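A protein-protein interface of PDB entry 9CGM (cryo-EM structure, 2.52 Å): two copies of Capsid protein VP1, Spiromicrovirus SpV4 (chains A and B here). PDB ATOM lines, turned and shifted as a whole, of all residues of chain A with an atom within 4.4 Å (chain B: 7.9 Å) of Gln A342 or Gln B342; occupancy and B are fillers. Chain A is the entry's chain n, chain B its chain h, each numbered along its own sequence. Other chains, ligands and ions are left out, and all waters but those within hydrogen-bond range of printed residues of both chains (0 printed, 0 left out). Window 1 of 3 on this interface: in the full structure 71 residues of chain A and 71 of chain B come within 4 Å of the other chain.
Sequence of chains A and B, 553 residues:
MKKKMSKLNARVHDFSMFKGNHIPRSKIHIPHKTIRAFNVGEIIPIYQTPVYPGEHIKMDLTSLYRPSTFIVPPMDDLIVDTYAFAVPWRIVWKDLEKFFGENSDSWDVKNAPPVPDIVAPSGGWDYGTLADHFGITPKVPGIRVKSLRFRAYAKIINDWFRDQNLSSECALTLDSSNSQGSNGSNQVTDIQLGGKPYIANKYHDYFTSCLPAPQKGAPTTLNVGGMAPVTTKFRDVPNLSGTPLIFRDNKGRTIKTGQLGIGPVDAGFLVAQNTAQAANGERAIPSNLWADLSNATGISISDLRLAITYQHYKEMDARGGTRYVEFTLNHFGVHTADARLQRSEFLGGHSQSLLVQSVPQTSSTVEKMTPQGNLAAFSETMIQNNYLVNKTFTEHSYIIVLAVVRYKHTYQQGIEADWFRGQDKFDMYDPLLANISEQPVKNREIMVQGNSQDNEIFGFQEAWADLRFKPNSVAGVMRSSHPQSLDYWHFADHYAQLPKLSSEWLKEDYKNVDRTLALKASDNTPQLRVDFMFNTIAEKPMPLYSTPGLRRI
Among the printed residues, pairs that only touch across the chains: Ala A339 with Arg B340 (3.5 Å), Arg A340 with Ala B339 (3.5 Å), Arg A90 with Leu B341 (3.8 Å) and Leu A341 with Arg B90 (3.8 Å).
The guanidinium group (NH1) of Arg B90 sits close to the side-chain amide nitrogen (NE2) of Gln B342. The side-chain amino group (NZ) of Lys B155 is in hydrogen-bond range of the backbone carbonyl oxygen (O) of Gln B342 (3.0 Å). The side-chain amino group (NZ) of Lys A155 is in hydrogen-bond range of the backbone carbonyl oxygen (O) of Gln A342, at 3.0 Å. NH1 of Arg A90 lies close to NE2 of Gln A342.
Hydrophobic or aromatic side chains of chain A within 4 Å of the printed part of chain B: Ala A339 and Leu A341. Among the printed residues, 8 pairs touch across the chains. Among the printed residues, Asp or Glu carboxylates within 4 Å of a Lys or Arg side-chain nitrogen of the other chain: Arg A340 with Glu B345 (2.6 Å).
Of the printed residues of chain B, Leu A341 touches Arg B90. Gln A342 touches just one residue of chain B: Gln B342. Printed residues of chain A within 4 Å of Arg B340: Arg A90 (2.7 Å) and Ala A339 (3.5 Å). Gln B342 touches one residue of chain A. The nearest residue of chain B that does not touch Gln A342 is Arg B90 (4.2 Å). The nearest printed residue of chain B that does not touch Ala A339 is Ala B339 (4.4 Å).
Arg A90 touches Arg B340, and with the chains exchanged Arg A340 touches Arg B90. Arg A90 touches Leu B341, and with the chains exchanged Leu A341 touches Arg B90. Ala A339 touches Arg B340, and with the chains exchanged Arg A340 touches Ala B339. Gln B342 touches its own counterpart, Gln A342. Positions printed for both chains: 90, 91, 155, 338, 339, 340, 341, 342, 343 and 344. Of the 8 pairs that touch across the chains among the printed residues, 7 have their exchanged pair printed and touching as well.
O of Arg B340 is in hydrogen-bond range of NH2 of Arg A90. NE2 of Gln B342 lies within hydrogen-bond range of OE1 of Gln A342 (2.9 Å). The side-chain carboxylate (OE2) of Glu B345 lies within salt-bridge range of the guanidinium group (NH2) of Arg A340 (2.6 Å). NH2 of Arg B90 is in hydrogen-bond range of O of Arg A340 (2.7 Å).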
ATOM      1  N   ARG A  90      32.875  32.491  31.175  1.00  0.00           N
ATOM      2  CA  ARG A  90      32.540  32.763  29.788  1.00  0.00           C
ATOM      3  C   ARG A  90      31.057  32.563  29.506  1.00  0.00           C
ATOM      4  O   ARG A  90      30.475  33.288  28.696  1.00  0.00           O
ATOM      5  CB  ARG A  90      33.383  31.858  28.913  1.00  0.00           C
ATOM      6  CG  ARG A  90      33.180  31.998  27.456  1.00  0.00           C
ATOM      7  CD  ARG A  90      34.038  30.973  26.781  1.00  0.00           C
ATOM      8  NE  ARG A  90      33.660  29.656  27.256  1.00  0.00           N
ATOM      9  CZ  ARG A  90      32.613  28.979  26.809  1.00  0.00           C
ATOM     10  NH1 ARG A  90      31.838  29.497  25.870  1.00  0.00           N
ATOM     11  NH2 ARG A  90      32.342  27.786  27.313  1.00  0.00           N
ATOM     12  N   ILE A  91      30.427  31.573  30.142  1.00  0.00           N
ATOM     13  CA  ILE A  91      28.998  31.361  29.925  1.00  0.00           C
ATOM     14  C   ILE A  91      28.139  32.305  30.745  1.00  0.00           C
ATOM     15  O   ILE A  91      26.945  32.440  30.468  1.00  0.00           O
ATOM     16  CB  ILE A  91      28.581  29.913  30.239  1.00  0.00           C
ATOM     17  CG1 ILE A  91      28.754  29.595  31.723  1.00  0.00           C
ATOM     18  CG2 ILE A  91      29.389  28.941  29.408  1.00  0.00           C
ATOM     19  CD1 ILE A  91      28.219  28.244  32.134  1.00  0.00           C
ATOM     20  N   LYS A 155      22.496  30.713  36.920  1.00  0.00           N
ATOM     21  CA  LYS A 155      22.785  29.769  35.851  1.00  0.00           C
ATOM     22  C   LYS A 155      22.641  28.328  36.324  1.00  0.00           C
ATOM     23  O   LYS A 155      22.150  27.473  35.583  1.00  0.00           O
ATOM     24  CB  LYS A 155      24.189  30.028  35.309  1.00  0.00           C
ATOM     25  CG  LYS A 155      24.674  29.077  34.225  1.00  0.00           C
ATOM     26  CD  LYS A 155      23.842  29.162  32.963  1.00  0.00           C
ATOM     27  CE  LYS A 155      24.468  28.357  31.853  1.00  0.00           C
ATOM     28  NZ  LYS A 155      23.591  28.231  30.681  1.00  0.00           N
ATOM     29  N   ASP A 338      27.875  18.577  28.841  1.00  0.00           N
ATOM     30  CA  ASP A 338      27.338  19.828  29.357  1.00  0.00           C
ATOM     31  C   ASP A 338      28.171  21.018  28.910  1.00  0.00           C
ATOM     32  O   ASP A 338      27.631  22.089  28.620  1.00  0.00           O
ATOM     33  CB  ASP A 338      27.279  19.770  30.884  1.00  0.00           C
ATOM     34  CG  ASP A 338      26.233  18.800  31.394  1.00  0.00           C
ATOM     35  OD1 ASP A 338      25.283  18.477  30.657  1.00  0.00           O
ATOM     36  OD2 ASP A 338      26.381  18.328  32.534  1.00  0.00           O
ATOM     37  N   ALA A 339      29.491  20.853  28.854  1.00  0.00           N
ATOM     38  CA  ALA A 339      30.356  21.966  28.498  1.00  0.00           C
ATOM     39  C   ALA A 339      30.230  22.325  27.027  1.00  0.00           C
ATOM     40  O   ALA A 339      30.345  23.499  26.667  1.00  0.00           O
ATOM     41  CB  ALA A 339      31.801  21.638  28.847  1.00  0.00           C
ATOM     42  N   ARG A 340      30.000  21.337  26.165  1.00  0.00           N
ATOM     43  CA  ARG A 340      29.723  21.630  24.766  1.00  0.00           C
ATOM     44  C   ARG A 340      28.501  22.522  24.621  1.00  0.00           C
ATOM     45  O   ARG A 340      28.478  23.428  23.786  1.00  0.00           O
ATOM     46  CB  ARG A 340      29.534  20.331  23.989  1.00  0.00           C
ATOM     47  CG  ARG A 340      29.183  20.533  22.537  1.00  0.00           C
ATOM     48  CD  ARG A 340      28.972  19.225  21.817  1.00  0.00           C
ATOM     49  NE  ARG A 340      30.217  18.509  21.593  1.00  0.00           N
ATOM     50  CZ  ARG A 340      30.994  18.698  20.538  1.00  0.00           C
ATOM     51  NH1 ARG A 340      30.644  19.573  19.615  1.00  0.00           N
ATOM     52  NH2 ARG A 340      32.114  18.013  20.406  1.00  0.00           N
ATOM     53  N   LEU A 341      27.487  22.295  25.442  1.00  0.00           N
ATOM     54  CA  LEU A 341      26.223  22.999  25.355  1.00  0.00           C
ATOM     55  C   LEU A 341      26.182  24.261  26.188  1.00  0.00           C
ATOM     56  O   LEU A 341      25.126  24.891  26.272  1.00  0.00           O
ATOM     57  CB  LEU A 341      25.092  22.079  25.778  1.00  0.00           C
ATOM     58  CG  LEU A 341      24.929  20.874  24.860  1.00  0.00           C
ATOM     59  CD1 LEU A 341      23.817  19.983  25.358  1.00  0.00           C
ATOM     60  CD2 LEU A 341      24.687  21.330  23.441  1.00  0.00           C
ATOM     61  N   GLN A 342      27.296  24.633  26.812  1.00  0.00           N
ATOM     62  CA  GLN A 342      27.383  25.820  27.654  1.00  0.00           C
ATOM     63  C   GLN A 342      26.461  25.735  28.861  1.00  0.00           C
ATOM     64  O   GLN A 342      25.741  26.677  29.182  1.00  0.00           O
ATOM     65  CB  GLN A 342      27.103  27.087  26.860  1.00  0.00           C
ATOM     66  CG  GLN A 342      28.209  27.500  25.968  1.00  0.00           C
ATOM     67  CD  GLN A 342      27.906  28.807  25.299  1.00  0.00           C
ATOM     68  OE1 GLN A 342      26.763  29.085  24.947  1.00  0.00           O
ATOM     69  NE2 GLN A 342      28.906  29.664  25.207  1.00  0.00           N
ATOM     70  N   ARG A 343      26.491  24.604  29.542  1.00  0.00           N
ATOM     71  CA  ARG A 343      25.802  24.438  30.805  1.00  0.00           C
ATOM     72  C   ARG A 343      26.842  24.346  31.909  1.00  0.00           C
ATOM     73  O   ARG A 343      27.983  23.946  31.674  1.00  0.00           O
ATOM     74  CB  ARG A 343      24.926  23.183  30.810  1.00  0.00           C
ATOM     75  CG  ARG A 343      23.870  23.144  29.741  1.00  0.00           C
ATOM     76  CD  ARG A 343      23.037  21.867  29.790  1.00  0.00           C
ATOM     77  NE  ARG A 343      22.124  21.806  30.934  1.00  0.00           N
ATOM     78  CZ  ARG A 343      22.212  20.925  31.924  1.00  0.00           C
ATOM     79  NH1 ARG A 343      23.161  20.011  31.916  1.00  0.00           N
ATOM     80  NH2 ARG A 343      21.342  20.949  32.913  1.00  0.00           N
ATOM     81  N   SER A 344      26.451  24.752  33.109  1.00  0.00           N
ATOM     82  CA  SER A 344      27.312  24.557  34.263  1.00  0.00           C
ATOM     83  C   SER A 344      27.537  23.071  34.504  1.00  0.00           C
ATOM     84  O   SER A 344      26.651  22.246  34.281  1.00  0.00           O
ATOM     85  CB  SER A 344      26.698  25.222  35.492  1.00  0.00           C
ATOM     86  OG  SER A 344      25.426  24.690  35.777  1.00  0.00           O
ATOM     87  N   PRO B  88      28.500  23.052  14.544  1.00  0.00           N
ATOM     88  CA  PRO B  88      27.168  22.898  15.129  1.00  0.00           C
ATOM     89  C   PRO B  88      26.247  24.029  14.710  1.00  0.00           C
ATOM     90  O   PRO B  88      26.642  25.193  14.687  1.00  0.00           O
ATOM     91  CB  PRO B  88      27.444  22.940  16.631  1.00  0.00           C
ATOM     92  CG  PRO B  88      28.833  22.529  16.757  1.00  0.00           C
ATOM     93  CD  PRO B  88      29.541  23.075  15.578  1.00  0.00           C
ATOM     94  N   ARG B  90      24.156  25.232  16.447  1.00  0.00           N
ATOM     95  CA  ARG B  90      23.922  26.005  17.655  1.00  0.00           C
ATOM     96  C   ARG B  90      24.868  27.193  17.768  1.00  0.00           C
ATOM     97  O   ARG B  90      24.481  28.250  18.272  1.00  0.00           O
ATOM     98  CB  ARG B  90      24.075  25.079  18.844  1.00  0.00           C
ATOM     99  CG  ARG B  90      23.866  25.694  20.171  1.00  0.00           C
ATOM    100  CD  ARG B  90      24.138  24.643  21.203  1.00  0.00           C
ATOM    101  NE  ARG B  90      25.495  24.160  21.038  1.00  0.00           N
ATOM    102  CZ  ARG B  90      26.566  24.790  21.494  1.00  0.00           C
ATOM    103  NH1 ARG B  90      26.438  25.932  22.148  1.00  0.00           N
ATOM    104  NH2 ARG B  90      27.767  24.276  21.283  1.00  0.00           N
ATOM    105  N   ILE B  91      26.119  27.043  17.329  1.00  0.00           N
ATOM    106  CA  ILE B  91      27.053  28.164  17.390  1.00  0.00           C
ATOM    107  C   ILE B  91      26.870  29.137  16.241  1.00  0.00           C
ATOM    108  O   ILE B  91      27.381  30.259  16.304  1.00  0.00           O
ATOM    109  CB  ILE B  91      28.518  27.687  17.408  1.00  0.00           C
ATOM    110  CG1 ILE B  91      28.893  26.999  16.096  1.00  0.00           C
ATOM    111  CG2 ILE B  91      28.750  26.744  18.567  1.00  0.00           C
ATOM    112  CD1 ILE B  91      30.356  26.644  15.979  1.00  0.00           C
ATOM    113  N   VAL B  92      26.194  28.722  15.177  1.00  0.00           N
ATOM    114  CA  VAL B  92      25.820  29.611  14.095  1.00  0.00           C
ATOM    115  C   VAL B  92      24.525  30.374  14.355  1.00  0.00           C
ATOM    116  O   VAL B  92      24.396  31.517  13.909  1.00  0.00           O
ATOM    117  CB  VAL B  92      25.749  28.817  12.773  1.00  0.00           C
ATOM    118  CG1 VAL B  92      24.895  29.494  11.773  1.00  0.00           C
ATOM    119  CG2 VAL B  92      27.134  28.717  12.201  1.00  0.00           C
ATOM    120  N   TRP B  93      23.567  29.792  15.062  1.00  0.00           N
ATOM    121  CA  TRP B  93      22.259  30.398  15.262  1.00  0.00           C
ATOM    122  C   TRP B  93      21.830  30.262  16.708  1.00  0.00           C
ATOM    123  O   TRP B  93      21.847  29.166  17.268  1.00  0.00           O
ATOM    124  CB  TRP B  93      21.243  29.793  14.287  1.00  0.00           C
ATOM    125  CG  TRP B  93      19.826  30.219  14.452  1.00  0.00           C
ATOM    126  CD1 TRP B  93      19.375  31.488  14.507  1.00  0.00           C
ATOM    127  CD2 TRP B  93      18.669  29.386  14.325  1.00  0.00           C
ATOM    128  NE1 TRP B  93      18.008  31.506  14.567  1.00  0.00           N
ATOM    129  CE2 TRP B  93      17.552  30.223  14.435  1.00  0.00           C
ATOM    130  CE3 TRP B  93      18.469  28.009  14.186  1.00  0.00           C
ATOM    131  CZ2 TRP B  93      16.251  29.734  14.397  1.00  0.00           C
ATOM    132  CZ3 TRP B  93      17.192  27.537  14.172  1.00  0.00           C
ATOM    133  CH2 TRP B  93      16.090  28.375  14.269  1.00  0.00           C
ATOM    134  N   GLU B  97      18.086  26.130  20.059  1.00  0.00           N
ATOM    135  CA  GLU B  97      17.430  25.405  21.144  1.00  0.00           C
ATOM    136  C   GLU B  97      15.954  25.758  21.225  1.00  0.00           C
ATOM    137  O   GLU B  97      15.110  24.892  21.476  1.00  0.00           O
ATOM    138  CB  GLU B  97      18.103  25.689  22.478  1.00  0.00           C
ATOM    139  CG  GLU B  97      19.515  25.188  22.619  1.00  0.00           C
ATOM    140  CD  GLU B  97      20.555  26.211  22.242  1.00  0.00           C
ATOM    141  OE1 GLU B  97      20.213  27.288  21.706  1.00  0.00           O
ATOM    142  OE2 GLU B  97      21.732  25.951  22.533  1.00  0.00           O
ATOM    143  N   LYS B 155      32.173  31.360   9.961  1.00  0.00           N
ATOM    144  CA  LYS B 155      32.636  30.920  11.269  1.00  0.00           C
ATOM    145  C   LYS B 155      33.965  30.182  11.170  1.00  0.00           C
ATOM    146  O   LYS B 155      34.834  30.342  12.031  1.00  0.00           O
ATOM    147  CB  LYS B 155      31.569  30.039  11.916  1.00  0.00           C
ATOM    148  CG  LYS B 155      31.929  29.437  13.268  1.00  0.00           C
ATOM    149  CD  LYS B 155      32.141  30.491  14.335  1.00  0.00           C
ATOM    150  CE  LYS B 155      32.298  29.854  15.691  1.00  0.00           C
ATOM    151  NZ  LYS B 155      32.722  30.814  16.720  1.00  0.00           N
ATOM    152  N   ASP B 159      37.507  31.297  12.961  1.00  0.00           N
ATOM    153  CA  ASP B 159      38.162  30.457  13.953  1.00  0.00           C
ATOM    154  C   ASP B 159      39.534  29.992  13.507  1.00  0.00           C
ATOM    155  O   ASP B 159      40.380  29.686  14.350  1.00  0.00           O
ATOM    156  CB  ASP B 159      37.313  29.230  14.277  1.00  0.00           C
ATOM    157  CG  ASP B 159      36.098  29.553  15.107  1.00  0.00           C
ATOM    158  OD1 ASP B 159      36.015  30.657  15.670  1.00  0.00           O
ATOM    159  OD2 ASP B 159      35.224  28.683  15.200  1.00  0.00           O
ATOM    160  N   LEU B 174      24.147  36.068  14.256  1.00  0.00           N
ATOM    161  CA  LEU B 174      23.591  34.927  14.963  1.00  0.00           C
ATOM    162  C   LEU B 174      22.075  34.961  15.073  1.00  0.00           C
ATOM    163  O   LEU B 174      21.488  34.006  15.574  1.00  0.00           O
ATOM    164  CB  LEU B 174      24.218  34.831  16.356  1.00  0.00           C
ATOM    165  CG  LEU B 174      25.743  34.713  16.338  1.00  0.00           C
ATOM    166  CD1 LEU B 174      26.316  34.717  17.740  1.00  0.00           C
ATOM    167  CD2 LEU B 174      26.198  33.498  15.576  1.00  0.00           C
ATOM    168  N   ALA B 337      39.434  22.606  24.866  1.00  0.00           N
ATOM    169  CA  ALA B 337      38.780  22.006  23.714  1.00  0.00           C
ATOM    170  C   ALA B 337      38.027  23.052  22.903  1.00  0.00           C
ATOM    171  O   ALA B 337      37.466  24.004  23.449  1.00  0.00           O
ATOM    172  CB  ALA B 337      37.827  20.904  24.162  1.00  0.00           C
ATOM    173  N   ASP B 338      38.014  22.859  21.585  1.00  0.00           N
ATOM    174  CA  ASP B 338      37.357  23.802  20.692  1.00  0.00           C
ATOM    175  C   ASP B 338      35.856  23.841  20.928  1.00  0.00           C
ATOM    176  O   ASP B 338      35.235  24.904  20.851  1.00  0.00           O
ATOM    177  CB  ASP B 338      37.652  23.427  19.240  1.00  0.00           C
ATOM    178  CG  ASP B 338      39.100  23.659  18.857  1.00  0.00           C
ATOM    179  OD1 ASP B 338      39.787  24.465  19.512  1.00  0.00           O
ATOM    180  OD2 ASP B 338      39.567  23.002  17.910  1.00  0.00           O
ATOM    181  N   ALA B 339      35.253  22.687  21.209  1.00  0.00           N
ATOM    182  CA  ALA B 339      33.810  22.637  21.383  1.00  0.00           C
ATOM    183  C   ALA B 339      33.377  23.304  22.677  1.00  0.00           C
ATOM    184  O   ALA B 339      32.299  23.900  22.732  1.00  0.00           O
ATOM    185  CB  ALA B 339      33.330  21.193  21.337  1.00  0.00           C
ATOM    186  N   ARG B 340      34.194  23.212  23.724  1.00  0.00           N
ATOM    187  CA  ARG B 340      33.908  23.951  24.946  1.00  0.00           C
ATOM    188  C   ARG B 340      33.832  25.445  24.681  1.00  0.00           C
ATOM    189  O   ARG B 340      32.983  26.141  25.241  1.00  0.00           O
ATOM    190  CB  ARG B 340      34.969  23.645  25.999  1.00  0.00           C
ATOM    191  CG  ARG B 340      34.793  24.412  27.285  1.00  0.00           C
ATOM    192  CD  ARG B 340      35.881  24.106  28.281  1.00  0.00           C
ATOM    193  NE  ARG B 340      35.748  22.778  28.857  1.00  0.00           N
ATOM    194  CZ  ARG B 340      35.013  22.509  29.925  1.00  0.00           C
ATOM    195  NH1 ARG B 340      34.359  23.481  30.531  1.00  0.00           N
ATOM    196  NH2 ARG B 340      34.937  21.275  30.386  1.00  0.00           N
ATOM    197  N   LEU B 341      34.696  25.950  23.814  1.00  0.00           N
ATOM    198  CA  LEU B 341      34.807  27.369  23.537  1.00  0.00           C
ATOM    199  C   LEU B 341      33.911  27.830  22.407  1.00  0.00           C
ATOM    200  O   LEU B 341      33.990  28.995  22.016  1.00  0.00           O
ATOM    201  CB  LEU B 341      36.246  27.718  23.213  1.00  0.00           C
ATOM    202  CG  LEU B 341      37.196  27.477  24.379  1.00  0.00           C
ATOM    203  CD1 LEU B 341      38.614  27.808  23.978  1.00  0.00           C
ATOM    204  CD2 LEU B 341      36.755  28.274  25.583  1.00  0.00           C
ATOM    205  N   GLN B 342      33.077  26.942  21.872  1.00  0.00           N
ATOM    206  CA  GLN B 342      32.174  27.257  20.771  1.00  0.00           C
ATOM    207  C   GLN B 342      32.924  27.658  19.511  1.00  0.00           C
ATOM    208  O   GLN B 342      32.595  28.646  18.858  1.00  0.00           O
ATOM    209  CB  GLN B 342      31.176  28.337  21.161  1.00  0.00           C
ATOM    210  CG  GLN B 342      30.098  27.872  22.062  1.00  0.00           C
ATOM    211  CD  GLN B 342      29.099  28.957  22.321  1.00  0.00           C
ATOM    212  OE1 GLN B 342      29.453  30.128  22.424  1.00  0.00           O
ATOM    213  NE2 GLN B 342      27.830  28.597  22.326  1.00  0.00           N
ATOM    214  N   ARG B 343      33.933  26.881  19.157  1.00  0.00           N
ATOM    215  CA  ARG B 343      34.629  27.035  17.897  1.00  0.00           C
ATOM    216  C   ARG B 343      34.285  25.850  17.013  1.00  0.00           C
ATOM    217  O   ARG B 343      33.947  24.770  17.501  1.00  0.00           O
ATOM    218  CB  ARG B 343      36.145  27.114  18.094  1.00  0.00           C
ATOM    219  CG  ARG B 343      36.610  28.238  18.978  1.00  0.00           C
ATOM    220  CD  ARG B 343      38.126  28.260  19.146  1.00  0.00           C
ATOM    221  NE  ARG B 343      38.843  28.682  17.939  1.00  0.00           N
ATOM    222  CZ  ARG B 343      39.657  27.904  17.234  1.00  0.00           C
ATOM    223  NH1 ARG B 343      39.881  26.662  17.613  1.00  0.00           N
ATOM    224  NH2 ARG B 343      40.259  28.375  16.161  1.00  0.00           N
ATOM    225  N   SER B 344      34.337  26.066  15.705  1.00  0.00           N
ATOM    226  CA  SER B 344      34.184  24.961  14.774  1.00  0.00           C
ATOM    227  C   SER B 344      35.313  23.958  14.961  1.00  0.00           C
ATOM    228  O   SER B 344      36.449  24.322  15.263  1.00  0.00           O
ATOM    229  CB  SER B 344      34.151  25.486  13.341  1.00  0.00           C
ATOM    230  OG  SER B 344      35.333  26.185  13.028  1.00  0.00           O
ATOM    231  N   GLU B 345      34.992  22.683  14.792  1.00  0.00           N
ATOM    232  CA  GLU B 345      35.923  21.607  15.082  1.00  0.00           C
ATOM    233  C   GLU B 345      36.684  21.219  13.825  1.00  0.00           C
ATOM    234  O   GLU B 345      36.086  21.019  12.769  1.00  0.00           O
ATOM    235  CB  GLU B 345      35.181  20.394  15.635  1.00  0.00           C
ATOM    236  CG  GLU B 345      34.512  20.617  16.981  1.00  0.00           C
ATOM    237  CD  GLU B 345      33.695  19.418  17.434  1.00  0.00           C
ATOM    238  OE1 GLU B 345      33.528  18.468  16.646  1.00  0.00           O
ATOM    239  OE2 GLU B 345      33.200  19.425  18.574  1.00  0.00           O
